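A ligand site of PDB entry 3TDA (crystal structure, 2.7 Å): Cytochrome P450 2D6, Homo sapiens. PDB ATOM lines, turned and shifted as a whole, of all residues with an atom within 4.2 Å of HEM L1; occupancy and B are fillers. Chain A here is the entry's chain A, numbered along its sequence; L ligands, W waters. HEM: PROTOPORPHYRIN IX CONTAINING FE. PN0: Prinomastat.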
ATOM      1  N   ARG A  79      34.741  20.782 -12.419  1.00  0.00           N
ATOM      2  CA  ARG A  79      35.002  19.989 -13.630  1.00  0.00           C
ATOM      3  C   ARG A  79      36.362  19.286 -13.482  1.00  0.00           C
ATOM      4  O   ARG A  79      37.186  19.647 -12.650  1.00  0.00           O
ATOM      5  CB  ARG A  79      35.092  20.877 -14.895  1.00  0.00           C
ATOM      6  CG  ARG A  79      33.856  21.692 -15.259  1.00  0.00           C
ATOM      7  CD  ARG A  79      32.727  20.845 -15.805  1.00  0.00           C
ATOM      8  NE  ARG A  79      31.639  21.699 -16.266  1.00  0.00           N
ATOM      9  CZ  ARG A  79      30.358  21.357 -16.310  1.00  0.00           C
ATOM     10  NH1 ARG A  79      29.455  22.223 -16.753  1.00  0.00           N
ATOM     11  NH2 ARG A  79      29.980  20.150 -15.912  1.00  0.00           N
ATOM     12  N   VAL A  97      33.401  29.268 -19.391  1.00  0.00           N
ATOM     13  CA  VAL A  97      32.361  28.816 -18.476  1.00  0.00           C
ATOM     14  C   VAL A  97      32.262  27.302 -18.469  1.00  0.00           C
ATOM     15  O   VAL A  97      32.492  26.657 -17.446  1.00  0.00           O
ATOM     16  CB  VAL A  97      30.972  29.437 -18.827  1.00  0.00           C
ATOM     17  CG1 VAL A  97      29.894  28.841 -17.941  1.00  0.00           C
ATOM     18  CG2 VAL A  97      31.007  30.934 -18.620  1.00  0.00           C
ATOM     19  N   PHE A  98      31.946  26.731 -19.623  1.00  0.00           N
ATOM     20  CA  PHE A  98      31.780  25.300 -19.771  1.00  0.00           C
ATOM     21  C   PHE A  98      32.891  24.432 -19.172  1.00  0.00           C
ATOM     22  O   PHE A  98      32.610  23.484 -18.459  1.00  0.00           O
ATOM     23  CB  PHE A  98      31.609  24.987 -21.253  1.00  0.00           C
ATOM     24  CG  PHE A  98      31.093  23.600 -21.530  1.00  0.00           C
ATOM     25  CD1 PHE A  98      29.742  23.303 -21.400  1.00  0.00           C
ATOM     26  CD2 PHE A  98      31.963  22.601 -21.976  1.00  0.00           C
ATOM     27  CE1 PHE A  98      29.253  22.020 -21.724  1.00  0.00           C
ATOM     28  CE2 PHE A  98      31.496  21.321 -22.301  1.00  0.00           C
ATOM     29  CZ  PHE A  98      30.134  21.028 -22.180  1.00  0.00           C
ATOM     30  N   TRP A 106      34.788  31.027 -12.710  1.00  0.00           N
ATOM     31  CA  TRP A 106      33.576  30.475 -13.297  1.00  0.00           C
ATOM     32  C   TRP A 106      32.363  31.294 -12.882  1.00  0.00           C
ATOM     33  O   TRP A 106      31.582  31.756 -13.718  1.00  0.00           O
ATOM     34  CB  TRP A 106      33.395  29.028 -12.837  1.00  0.00           C
ATOM     35  CG  TRP A 106      32.017  28.475 -13.057  1.00  0.00           C
ATOM     36  CD1 TRP A 106      31.532  27.937 -14.205  1.00  0.00           C
ATOM     37  CD2 TRP A 106      30.934  28.489 -12.122  1.00  0.00           C
ATOM     38  NE1 TRP A 106      30.209  27.617 -14.050  1.00  0.00           N
ATOM     39  CE2 TRP A 106      29.812  27.950 -12.785  1.00  0.00           C
ATOM     40  CE3 TRP A 106      30.784  28.915 -10.791  1.00  0.00           C
ATOM     41  CZ2 TRP A 106      28.560  27.814 -12.163  1.00  0.00           C
ATOM     42  CZ3 TRP A 106      29.545  28.785 -10.169  1.00  0.00           C
ATOM     43  CH2 TRP A 106      28.450  28.240 -10.855  1.00  0.00           C
ATOM     44  N   ARG A 110      29.783  32.967 -15.217  1.00  0.00           N
ATOM     45  CA  ARG A 110      28.460  32.339 -15.138  1.00  0.00           C
ATOM     46  C   ARG A 110      27.370  33.396 -14.921  1.00  0.00           C
ATOM     47  O   ARG A 110      26.400  33.486 -15.675  1.00  0.00           O
ATOM     48  CB  ARG A 110      28.440  31.364 -13.953  1.00  0.00           C
ATOM     49  CG  ARG A 110      27.070  30.780 -13.590  1.00  0.00           C
ATOM     50  CD  ARG A 110      26.624  29.782 -14.636  1.00  0.00           C
ATOM     51  NE  ARG A 110      25.262  29.337 -14.395  1.00  0.00           N
ATOM     52  CZ  ARG A 110      24.756  28.193 -14.860  1.00  0.00           C
ATOM     53  NH1 ARG A 110      25.510  27.369 -15.575  1.00  0.00           N
ATOM     54  NH2 ARG A 110      23.490  27.900 -14.645  1.00  0.00           N
ATOM     55  N   ILE A 164      22.561  33.057 -31.726  1.00  0.00           N
ATOM     56  CA  ILE A 164      23.548  33.257 -30.697  1.00  0.00           C
ATOM     57  C   ILE A 164      24.570  34.311 -31.126  1.00  0.00           C
ATOM     58  O   ILE A 164      25.014  35.114 -30.301  1.00  0.00           O
ATOM     59  CB  ILE A 164      24.252  31.930 -30.286  1.00  0.00           C
ATOM     60  CG1 ILE A 164      25.108  32.166 -29.039  1.00  0.00           C
ATOM     61  CG2 ILE A 164      25.071  31.382 -31.433  1.00  0.00           C
ATOM     62  CD1 ILE A 164      24.317  32.646 -27.835  1.00  0.00           C
ATOM     63  N   ASP A 279      32.699  30.154 -26.140  1.00  0.00           N
ATOM     64  CA  ASP A 279      31.993  29.210 -25.293  1.00  0.00           C
ATOM     65  C   ASP A 279      30.495  29.227 -25.613  1.00  0.00           C
ATOM     66  O   ASP A 279      29.898  28.196 -25.902  1.00  0.00           O
ATOM     67  CB  ASP A 279      32.228  29.601 -23.834  1.00  0.00           C
ATOM     68  CG  ASP A 279      32.148  28.433 -22.906  1.00  0.00           C
ATOM     69  OD1 ASP A 279      31.046  27.869 -22.814  1.00  0.00           O
ATOM     70  OD2 ASP A 279      33.167  28.080 -22.285  1.00  0.00           O
ATOM     71  N   LEU A 280      29.929  30.425 -25.597  1.00  0.00           N
ATOM     72  CA  LEU A 280      28.515  30.617 -25.846  1.00  0.00           C
ATOM     73  C   LEU A 280      28.144  30.366 -27.305  1.00  0.00           C
ATOM     74  O   LEU A 280      27.128  29.715 -27.597  1.00  0.00           O
ATOM     75  CB  LEU A 280      28.122  32.035 -25.405  1.00  0.00           C
ATOM     76  CG  LEU A 280      28.396  32.335 -23.912  1.00  0.00           C
ATOM     77  CD1 LEU A 280      27.947  33.736 -23.540  1.00  0.00           C
ATOM     78  CD2 LEU A 280      27.671  31.350 -23.029  1.00  0.00           C
ATOM     79  N   ALA A 283      28.501  26.577 -28.163  1.00  0.00           N
ATOM     80  CA  ALA A 283      27.429  25.849 -27.500  1.00  0.00           C
ATOM     81  C   ALA A 283      26.105  26.084 -28.246  1.00  0.00           C
ATOM     82  O   ALA A 283      25.305  25.169 -28.422  1.00  0.00           O
ATOM     83  CB  ALA A 283      27.335  26.306 -26.057  1.00  0.00           C
ATOM     84  N   GLY A 284      25.886  27.320 -28.687  1.00  0.00           N
ATOM     85  CA  GLY A 284      24.670  27.653 -29.397  1.00  0.00           C
ATOM     86  C   GLY A 284      24.582  27.225 -30.852  1.00  0.00           C
ATOM     87  O   GLY A 284      23.498  27.289 -31.439  1.00  0.00           O
ATOM     88  N   THR A 287      23.773  22.641 -30.431  1.00  0.00           N
ATOM     89  CA  THR A 287      22.801  22.011 -29.538  1.00  0.00           C
ATOM     90  C   THR A 287      21.373  22.062 -30.061  1.00  0.00           C
ATOM     91  O   THR A 287      20.819  21.042 -30.463  1.00  0.00           O
ATOM     92  CB  THR A 287      22.827  22.682 -28.174  1.00  0.00           C
ATOM     93  OG1 THR A 287      22.646  24.106 -28.346  1.00  0.00           O
ATOM     94  CG2 THR A 287      24.154  22.365 -27.460  1.00  0.00           C
ATOM     95  N   THR A 288      20.798  23.263 -30.053  1.00  0.00           N
ATOM     96  CA  THR A 288      19.435  23.510 -30.532  1.00  0.00           C
ATOM     97  C   THR A 288      19.133  23.066 -31.983  1.00  0.00           C
ATOM     98  O   THR A 288      18.043  22.556 -32.280  1.00  0.00           O
ATOM     99  CB  THR A 288      19.096  24.994 -30.430  1.00  0.00           C
ATOM    100  OG1 THR A 288      19.264  25.420 -29.083  1.00  0.00           O
ATOM    101  CG2 THR A 288      17.667  25.229 -30.814  1.00  0.00           C
ATOM    102  N   THR A 291      18.742  19.382 -31.888  1.00  0.00           N
ATOM    103  CA  THR A 291      17.428  19.028 -31.394  1.00  0.00           C
ATOM    104  C   THR A 291      16.432  19.258 -32.542  1.00  0.00           C
ATOM    105  O   THR A 291      15.582  18.410 -32.785  1.00  0.00           O
ATOM    106  CB  THR A 291      17.000  19.897 -30.190  1.00  0.00           C
ATOM    107  OG1 THR A 291      17.946  19.746 -29.128  1.00  0.00           O
ATOM    108  CG2 THR A 291      15.619  19.503 -29.707  1.00  0.00           C
ATOM    109  N   GLN A 342      13.051  16.511 -27.348  1.00  0.00           N
ATOM    110  CA  GLN A 342      14.223  16.631 -26.507  1.00  0.00           C
ATOM    111  C   GLN A 342      14.431  15.354 -25.707  1.00  0.00           C
ATOM    112  O   GLN A 342      15.551  14.854 -25.622  1.00  0.00           O
ATOM    113  CB  GLN A 342      14.069  17.802 -25.553  1.00  0.00           C
ATOM    114  CG  GLN A 342      14.303  19.148 -26.183  1.00  0.00           C
ATOM    115  CD  GLN A 342      14.611  20.213 -25.148  1.00  0.00           C
ATOM    116  OE1 GLN A 342      13.688  20.777 -24.549  1.00  0.00           O
ATOM    117  NE2 GLN A 342      15.911  20.470 -24.904  1.00  0.00           N
ATOM    118  N   ILE A 347      20.041  14.216 -26.857  1.00  0.00           N
ATOM    119  CA  ILE A 347      21.223  14.701 -27.555  1.00  0.00           C
ATOM    120  C   ILE A 347      22.506  14.714 -26.738  1.00  0.00           C
ATOM    121  O   ILE A 347      23.590  14.730 -27.314  1.00  0.00           O
ATOM    122  CB  ILE A 347      21.003  16.063 -28.240  1.00  0.00           C
ATOM    123  CG1 ILE A 347      21.181  17.208 -27.254  1.00  0.00           C
ATOM    124  CG2 ILE A 347      19.647  16.129 -28.898  1.00  0.00           C
ATOM    125  CD1 ILE A 347      21.587  18.500 -27.905  1.00  0.00           C
ATOM    126  N   VAL A 348      22.401  14.747 -25.428  1.00  0.00           N
ATOM    127  CA  VAL A 348      23.582  14.758 -24.583  1.00  0.00           C
ATOM    128  C   VAL A 348      23.386  13.629 -23.579  1.00  0.00           C
ATOM    129  O   VAL A 348      23.182  13.869 -22.403  1.00  0.00           O
ATOM    130  CB  VAL A 348      23.702  16.076 -23.830  1.00  0.00           C
ATOM    131  CG1 VAL A 348      25.079  16.202 -23.227  1.00  0.00           C
ATOM    132  CG2 VAL A 348      23.427  17.222 -24.766  1.00  0.00           C
ATOM    133  N   VAL A 352      27.765  16.255 -19.196  1.00  0.00           N
ATOM    134  CA  VAL A 352      29.112  16.791 -19.189  1.00  0.00           C
ATOM    135  C   VAL A 352      29.704  16.371 -17.846  1.00  0.00           C
ATOM    136  O   VAL A 352      29.048  16.497 -16.795  1.00  0.00           O
ATOM    137  CB  VAL A 352      29.074  18.323 -19.326  1.00  0.00           C
ATOM    138  CG1 VAL A 352      30.496  18.883 -19.371  1.00  0.00           C
ATOM    139  CG2 VAL A 352      28.309  18.693 -20.581  1.00  0.00           C
ATOM    140  N   HIS A 354      31.566  15.909 -14.345  1.00  0.00           N
ATOM    141  CA  HIS A 354      31.679  16.720 -13.140  1.00  0.00           C
ATOM    142  C   HIS A 354      32.826  16.059 -12.341  1.00  0.00           C
ATOM    143  O   HIS A 354      33.373  15.020 -12.738  1.00  0.00           O
ATOM    144  CB  HIS A 354      30.410  16.647 -12.294  1.00  0.00           C
ATOM    145  CG  HIS A 354      29.303  17.537 -12.748  1.00  0.00           C
ATOM    146  ND1 HIS A 354      29.031  18.737 -12.146  1.00  0.00           N
ATOM    147  CD2 HIS A 354      28.367  17.377 -13.715  1.00  0.00           C
ATOM    148  CE1 HIS A 354      27.962  19.278 -12.695  1.00  0.00           C
ATOM    149  NE2 HIS A 354      27.531  18.466 -13.653  1.00  0.00           N
ATOM    150  N   LEU A 377      22.339  11.265 -18.191  1.00  0.00           N
ATOM    151  CA  LEU A 377      21.058  11.909 -18.496  1.00  0.00           C
ATOM    152  C   LEU A 377      20.127  10.985 -19.291  1.00  0.00           C
ATOM    153  O   LEU A 377      18.920  10.948 -19.074  1.00  0.00           O
ATOM    154  CB  LEU A 377      21.311  13.202 -19.268  1.00  0.00           C
ATOM    155  CG  LEU A 377      22.095  14.256 -18.452  1.00  0.00           C
ATOM    156  CD1 LEU A 377      22.227  15.536 -19.237  1.00  0.00           C
ATOM    157  CD2 LEU A 377      21.366  14.522 -17.142  1.00  0.00           C
ATOM    158  N   PRO A 413      17.055  17.200 -19.644  1.00  0.00           N
ATOM    159  CA  PRO A 413      17.909  17.290 -20.821  1.00  0.00           C
ATOM    160  C   PRO A 413      19.065  18.224 -20.538  1.00  0.00           C
ATOM    161  O   PRO A 413      20.110  18.129 -21.148  1.00  0.00           O
ATOM    162  CB  PRO A 413      16.973  17.882 -21.879  1.00  0.00           C
ATOM    163  CG  PRO A 413      15.853  18.490 -21.117  1.00  0.00           C
ATOM    164  CD  PRO A 413      15.681  17.607 -19.936  1.00  0.00           C
ATOM    165  N   PHE A 414      18.842  19.159 -19.633  1.00  0.00           N
ATOM    166  CA  PHE A 414      19.808  20.215 -19.318  1.00  0.00           C
ATOM    167  C   PHE A 414      20.591  19.964 -18.046  1.00  0.00           C
ATOM    168  O   PHE A 414      21.360  20.814 -17.604  1.00  0.00           O
ATOM    169  CB  PHE A 414      19.107  21.567 -19.167  1.00  0.00           C
ATOM    170  CG  PHE A 414      18.358  22.013 -20.393  1.00  0.00           C
ATOM    171  CD1 PHE A 414      16.977  21.896 -20.447  1.00  0.00           C
ATOM    172  CD2 PHE A 414      19.051  22.476 -21.512  1.00  0.00           C
ATOM    173  CE1 PHE A 414      16.284  22.250 -21.589  1.00  0.00           C
ATOM    174  CE2 PHE A 414      18.369  22.840 -22.674  1.00  0.00           C
ATOM    175  CZ  PHE A 414      16.985  22.712 -22.720  1.00  0.00           C
ATOM    176  N   SER A 415      20.398  18.799 -17.442  1.00  0.00           N
ATOM    177  CA  SER A 415      21.058  18.462 -16.184  1.00  0.00           C
ATOM    178  C   SER A 415      20.465  19.297 -15.033  1.00  0.00           C
ATOM    179  O   SER A 415      19.375  19.879 -15.169  1.00  0.00           O
ATOM    180  CB  SER A 415      22.565  18.674 -16.287  1.00  0.00           C
ATOM    181  OG  SER A 415      23.194  18.090 -15.174  1.00  0.00           O
ATOM    182  N   ARG A 419      25.547  24.087 -12.118  1.00  0.00           N
ATOM    183  CA  ARG A 419      26.188  23.941 -13.405  1.00  0.00           C
ATOM    184  C   ARG A 419      25.226  23.632 -14.553  1.00  0.00           C
ATOM    185  O   ARG A 419      25.653  23.517 -15.697  1.00  0.00           O
ATOM    186  CB  ARG A 419      27.238  22.839 -13.322  1.00  0.00           C
ATOM    187  CG  ARG A 419      28.502  23.242 -12.618  1.00  0.00           C
ATOM    188  CD  ARG A 419      29.288  24.185 -13.492  1.00  0.00           C
ATOM    189  NE  ARG A 419      30.660  24.212 -13.025  1.00  0.00           N
ATOM    190  CZ  ARG A 419      31.726  24.446 -13.780  1.00  0.00           C
ATOM    191  NH1 ARG A 419      31.617  24.703 -15.072  1.00  0.00           N
ATOM    192  NH2 ARG A 419      32.913  24.415 -13.216  1.00  0.00           N
ATOM    193  N   ALA A 420      23.931  23.487 -14.263  1.00  0.00           N
ATOM    194  CA  ALA A 420      22.984  23.163 -15.334  1.00  0.00           C
ATOM    195  C   ALA A 420      23.104  24.192 -16.448  1.00  0.00           C
ATOM    196  O   ALA A 420      23.439  25.344 -16.193  1.00  0.00           O
ATOM    197  CB  ALA A 420      21.549  23.119 -14.806  1.00  0.00           C
ATOM    198  N   CYS A 421      22.835  23.730 -17.662  1.00  0.00           N
ATOM    199  CA  CYS A 421      22.927  24.537 -18.878  1.00  0.00           C
ATOM    200  C   CYS A 421      22.412  25.914 -18.646  1.00  0.00           C
ATOM    201  O   CYS A 421      21.287  26.070 -18.153  1.00  0.00           O
ATOM    202  CB  CYS A 421      22.122  23.909 -20.004  1.00  0.00           C
ATOM    203  SG  CYS A 421      22.349  24.733 -21.623  1.00  0.00           S
ATOM    204  N   LEU A 422      23.210  26.924 -18.984  1.00  0.00           N
ATOM    205  CA  LEU A 422      22.771  28.292 -18.790  1.00  0.00           C
ATOM    206  C   LEU A 422      22.056  28.750 -20.036  1.00  0.00           C
ATOM    207  O   LEU A 422      21.455  29.817 -20.067  1.00  0.00           O
ATOM    208  CB  LEU A 422      23.933  29.230 -18.466  1.00  0.00           C
ATOM    209  CG  LEU A 422      25.014  29.605 -19.466  1.00  0.00           C
ATOM    210  CD1 LEU A 422      24.487  30.638 -20.450  1.00  0.00           C
ATOM    211  CD2 LEU A 422      26.162  30.202 -18.735  1.00  0.00           C
ATOM    212  N   GLY A 423      22.090  27.902 -21.066  1.00  0.00           N
ATOM    213  CA  GLY A 423      21.423  28.239 -22.304  1.00  0.00           C
ATOM    214  C   GLY A 423      19.998  27.715 -22.374  1.00  0.00           C
ATOM    215  O   GLY A 423      19.333  27.877 -23.405  1.00  0.00           O
ATOM    216  N   LEU A 426      17.290  30.248 -23.448  1.00  0.00           N
ATOM    217  CA  LEU A 426      17.450  30.510 -24.882  1.00  0.00           C
ATOM    218  C   LEU A 426      17.004  29.297 -25.726  1.00  0.00           C
ATOM    219  O   LEU A 426      16.367  29.452 -26.769  1.00  0.00           O
ATOM    220  CB  LEU A 426      18.897  30.853 -25.204  1.00  0.00           C
ATOM    221  CG  LEU A 426      19.256  31.054 -26.672  1.00  0.00           C
ATOM    222  CD1 LEU A 426      18.406  32.186 -27.272  1.00  0.00           C
ATOM    223  CD2 LEU A 426      20.764  31.341 -26.784  1.00  0.00           C
ATOM    224  N   ALA A 427      17.362  28.100 -25.280  1.00  0.00           N
ATOM    225  CA  ALA A 427      16.982  26.882 -25.998  1.00  0.00           C
ATOM    226  C   ALA A 427      15.461  26.728 -26.068  1.00  0.00           C
ATOM    227  O   ALA A 427      14.921  26.389 -27.141  1.00  0.00           O
ATOM    228  CB  ALA A 427      17.607  25.646 -25.336  1.00  0.00           C
HETATM  229  CHA HEM L   1      26.007  23.162 -20.124  1.00  0.00           C
HETATM  230  CHB HEM L   1      22.675  20.742 -22.478  1.00  0.00           C
HETATM  231  CHC HEM L   1      21.989  24.478 -25.241  1.00  0.00           C
HETATM  232  CHD HEM L   1      25.398  26.841 -22.973  1.00  0.00           C
HETATM  233  C1A HEM L   1      25.069  22.176 -20.391  1.00  0.00           C
HETATM  234  C2A HEM L   1      25.053  20.884 -19.830  1.00  0.00           C
HETATM  235  C3A HEM L   1      24.152  20.166 -20.566  1.00  0.00           C
HETATM  236  C4A HEM L   1      23.641  21.044 -21.544  1.00  0.00           C
HETATM  237  CMA HEM L   1      23.760  18.648 -20.355  1.00  0.00           C
HETATM  238  CAA HEM L   1      25.891  20.404 -18.646  1.00  0.00           C
HETATM  239  CBA HEM L   1      25.308  20.575 -17.290  1.00  0.00           C
HETATM  240  CGA HEM L   1      26.216  19.990 -16.218  1.00  0.00           C
HETATM  241  O1A HEM L   1      27.395  20.328 -16.136  1.00  0.00           O
HETATM  242  O2A HEM L   1      25.788  19.125 -15.451  1.00  0.00           O
HETATM  243  C1B HEM L   1      22.165  21.480 -23.527  1.00  0.00           C
HETATM  244  C2B HEM L   1      21.094  21.120 -24.401  1.00  0.00           C
HETATM  245  C3B HEM L   1      20.908  22.247 -25.245  1.00  0.00           C
HETATM  246  C4B HEM L   1      21.877  23.190 -24.794  1.00  0.00           C
HETATM  247  CMB HEM L   1      20.373  19.808 -24.397  1.00  0.00           C
HETATM  248  CAB HEM L   1      19.994  22.459 -26.289  1.00  0.00           C
HETATM  249  CBB HEM L   1      18.661  21.896 -26.545  1.00  0.00           C
HETATM  250  C1C HEM L   1      22.980  25.439 -25.084  1.00  0.00           C
HETATM  251  C2C HEM L   1      22.856  26.770 -25.507  1.00  0.00           C
HETATM  252  C3C HEM L   1      23.781  27.504 -24.790  1.00  0.00           C
HETATM  253  C4C HEM L   1      24.428  26.577 -23.952  1.00  0.00           C
HETATM  254  CMC HEM L   1      21.849  27.313 -26.588  1.00  0.00           C
HETATM  255  CAC HEM L   1      24.062  28.865 -24.814  1.00  0.00           C
HETATM  256  CBC HEM L   1      25.151  29.561 -25.341  1.00  0.00           C
HETATM  257  C1D HEM L   1      25.942  26.023 -22.050  1.00  0.00           C
HETATM  258  C2D HEM L   1      26.930  26.405 -21.136  1.00  0.00           C
HETATM  259  C3D HEM L   1      27.103  25.364 -20.268  1.00  0.00           C
HETATM  260  C4D HEM L   1      26.196  24.380 -20.720  1.00  0.00           C
HETATM  261  CMD HEM L   1      27.708  27.745 -21.089  1.00  0.00           C
HETATM  262  CAD HEM L   1      28.080  25.292 -19.066  1.00  0.00           C
HETATM  263  CBD HEM L   1      27.469  25.792 -17.730  1.00  0.00           C
HETATM  264  CGD HEM L   1      28.379  25.755 -16.476  1.00  0.00           C
HETATM  265  O1D HEM L   1      28.195  26.495 -15.543  1.00  0.00           O
HETATM  266  O2D HEM L   1      29.290  24.936 -16.433  1.00  0.00           O
HETATM  267  NA  HEM L   1      24.192  22.239 -21.440  1.00  0.00           N
HETATM  268  NB  HEM L   1      22.600  22.716 -23.794  1.00  0.00           N
HETATM  269  NC  HEM L   1      23.919  25.316 -24.149  1.00  0.00           N
HETATM  270  ND  HEM L   1      25.526  24.812 -21.781  1.00  0.00           N
HETATM  271 FE   HEM L   1      24.069  23.751 -22.830  1.00  0.00          FE
HETATM  272  N1  PN0 L   2      34.833  23.983 -26.774  1.00  0.00           N
HETATM  273  N3  PN0 L   2      32.115  25.505 -25.523  1.00  0.00           N
HETATM  274  C4  PN0 L   2      37.176  24.318 -25.859  1.00  0.00           C
HETATM  275  C5  PN0 L   2      32.472  22.530 -27.326  1.00  0.00           C
HETATM  276  C6  PN0 L   2      32.390  21.735 -26.150  1.00  0.00           C
HETATM  277  C7  PN0 L   2      31.139  21.274 -25.727  1.00  0.00           C
HETATM  278  C8  PN0 L   2      29.971  21.608 -26.482  1.00  0.00           C
HETATM  279  C10 PN0 L   2      31.301  22.884 -28.067  1.00  0.00           C
HETATM  280  C13 PN0 L   2      25.655  21.387 -24.403  1.00  0.00           C
HETATM  281  C15 PN0 L   2      27.818  23.100 -24.842  1.00  0.00           C
HETATM  282  C17 PN0 L   2      35.030  27.825 -26.346  1.00  0.00           C
HETATM  283  C1  PN0 L   2      35.550  26.393 -26.575  1.00  0.00           C
HETATM  284  C2  PN0 L   2      34.340  25.378 -26.572  1.00  0.00           C
HETATM  285  C3  PN0 L   2      35.950  23.396 -25.972  1.00  0.00           C
HETATM  286  S1  PN0 L   2      36.801  26.008 -25.358  1.00  0.00           S
HETATM  287  S2  PN0 L   2      34.022  23.045 -27.854  1.00  0.00           S
HETATM  288  C9  PN0 L   2      30.061  22.419 -27.636  1.00  0.00           C
HETATM  289  O1  PN0 L   2      28.744  21.148 -26.132  1.00  0.00           O
HETATM  290  C11 PN0 L   2      27.812  21.761 -25.383  1.00  0.00           C
HETATM  291  C12 PN0 L   2      26.733  20.908 -25.153  1.00  0.00           C
HETATM  292  N2  PN0 L   2      25.642  22.640 -23.883  1.00  0.00           N
HETATM  293  C14 PN0 L   2      26.688  23.480 -24.092  1.00  0.00           C
HETATM  294  O2  PN0 L   2      34.744  21.807 -27.949  1.00  0.00           O
HETATM  295  O3  PN0 L   2      33.853  23.831 -29.074  1.00  0.00           O
HETATM  296  C16 PN0 L   2      33.445  25.429 -25.311  1.00  0.00           C
HETATM  297  O4  PN0 L   2      31.162  25.559 -24.480  1.00  0.00           O
HETATM  298  O5  PN0 L   2      33.941  25.392 -24.168  1.00  0.00           O
HETATM  299  C18 PN0 L   2      36.152  26.447 -28.002  1.00  0.00           C
HETATM  300  O   HOH W   1      17.241  18.799 -26.447  1.00  0.00           O
HETATM  301  O   HOH W   2      25.551  16.775 -17.239  1.00  0.00           O
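Val 97 touches HEM L1.
CD1 of Phe 98 touches CAD of HEM L1, 3.5 Å away.
Asp 279 touches HEM L1 (OD1 to CMD, 3.8 Å).
Leu 280 touches HEM L1 (O to CBC, 3.0 Å).
Ala 283 touches HEM L1.
Gly 284 touches HEM L1 (CA to CMC, 3.996 Å).
Thr 287 touches HEM L1 (OG1 to CHC, 3.2 Å).
N of Thr 288 touches CAB of HEM L1, at 3.9 Å.
Thr 291 touches HEM L1.
Gln 342 touches HEM L1.
Ile 347 touches HEM L1.
Val 348 touches HEM L1 (CG1 to CMA, 3.996 Å).
Val 352 touches HEM L1.
Leu 377 touches HEM L1.
Pro 413 touches HEM L1 (O to CMB, 3.7 Å).
CE2 of Phe 414 touches C2B of HEM L1, 3.7 Å away.
Ala 420 touches HEM L1 (CA to CBA, 3.99 Å).
Leu 422 touches HEM L1.
Gly 423 touches HEM L1.
The nearest printed residue that does not touch HEM L1 is Ile 164 (4.1 Å).
A nitrogen (N2) of PN0 L2 binds an iron atom (FE) of HEM L1 (2.2 Å).
OG1 of Thr 291 sits at hydrogen-bond distance from O of Thr 287 (3.4 Å).
The guanidinium group of Arg 110 lies within hydrogen-bond range of the backbone carbonyl oxygen of Ala 420.
NE of Arg 79 sits at hydrogen-bond distance from O of Phe 98 (3.0 Å).
The backbone NH (N) of Cys 421 sits at hydrogen-bond distance from the backbone carbonyl oxygen (O) of Phe 414, at 3.3 Å.
The backbone NH of Val 97 sits at hydrogen-bond distance from the side-chain carboxylate of Asp 279, 3.1 Å away.
SG of Cys 421 sits close to N of Gly 423, 3.2 Å away.
The backbone carbonyl oxygen (O) of Ala 283 lies within hydrogen-bond range of the side-chain hydroxyl (OG1) of Thr 287 (2.9 Å).
The backbone carbonyl oxygen (O) of Val 97 is in hydrogen-bond range of the guanidinium group (NH1) of Arg 419 (3.2 Å).
Water W2 lies within hydrogen-bond range of an oxygen (O2A) of HEM L1 (3.0 Å), the backbone NH of Val 352 (3.0 Å) and the side-chain hydroxyl of Ser 415 (3.4 Å).
Water W1 bridges the side-chain amide nitrogen of Gln 342 (2.6 Å) and the side-chain hydroxyl of Thr 291 (2.9 Å).
NE1 of Trp 106 sits at hydrogen-bond distance from O1D of HEM L1 (2.7 Å).
An oxygen (O1D) of HEM L1 lies within salt-bridge range of the guanidinium group (NH1) of Arg 110 (2.8 Å).
A ring nitrogen (NE2) of His 354 is in hydrogen-bond range of an oxygen (O2A) of HEM L1 (2.6 Å).
O4 of PN0 L2 lies within hydrogen-bond range of OD1 of Asp 279.
An oxygen (O4) of PN0 L2 sits at hydrogen-bond distance from the backbone carbonyl oxygen (O) of Asp 279 (3.3 Å).
The guanidinium group of Arg 79 is in salt-bridge range of an oxygen (O1A) of HEM L1.
The side-chain sulfur of Cys 421 binds an iron atom (FE) of HEM L1, 2.3 Å away.
An oxygen (O2D) of HEM L1 is in salt-bridge range of the guanidinium group of Arg 419, at 2.7 Å.
The side-chain hydroxyl of Ser 415 sits at hydrogen-bond distance from an oxygen (O2A) of HEM L1 (2.8 Å).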
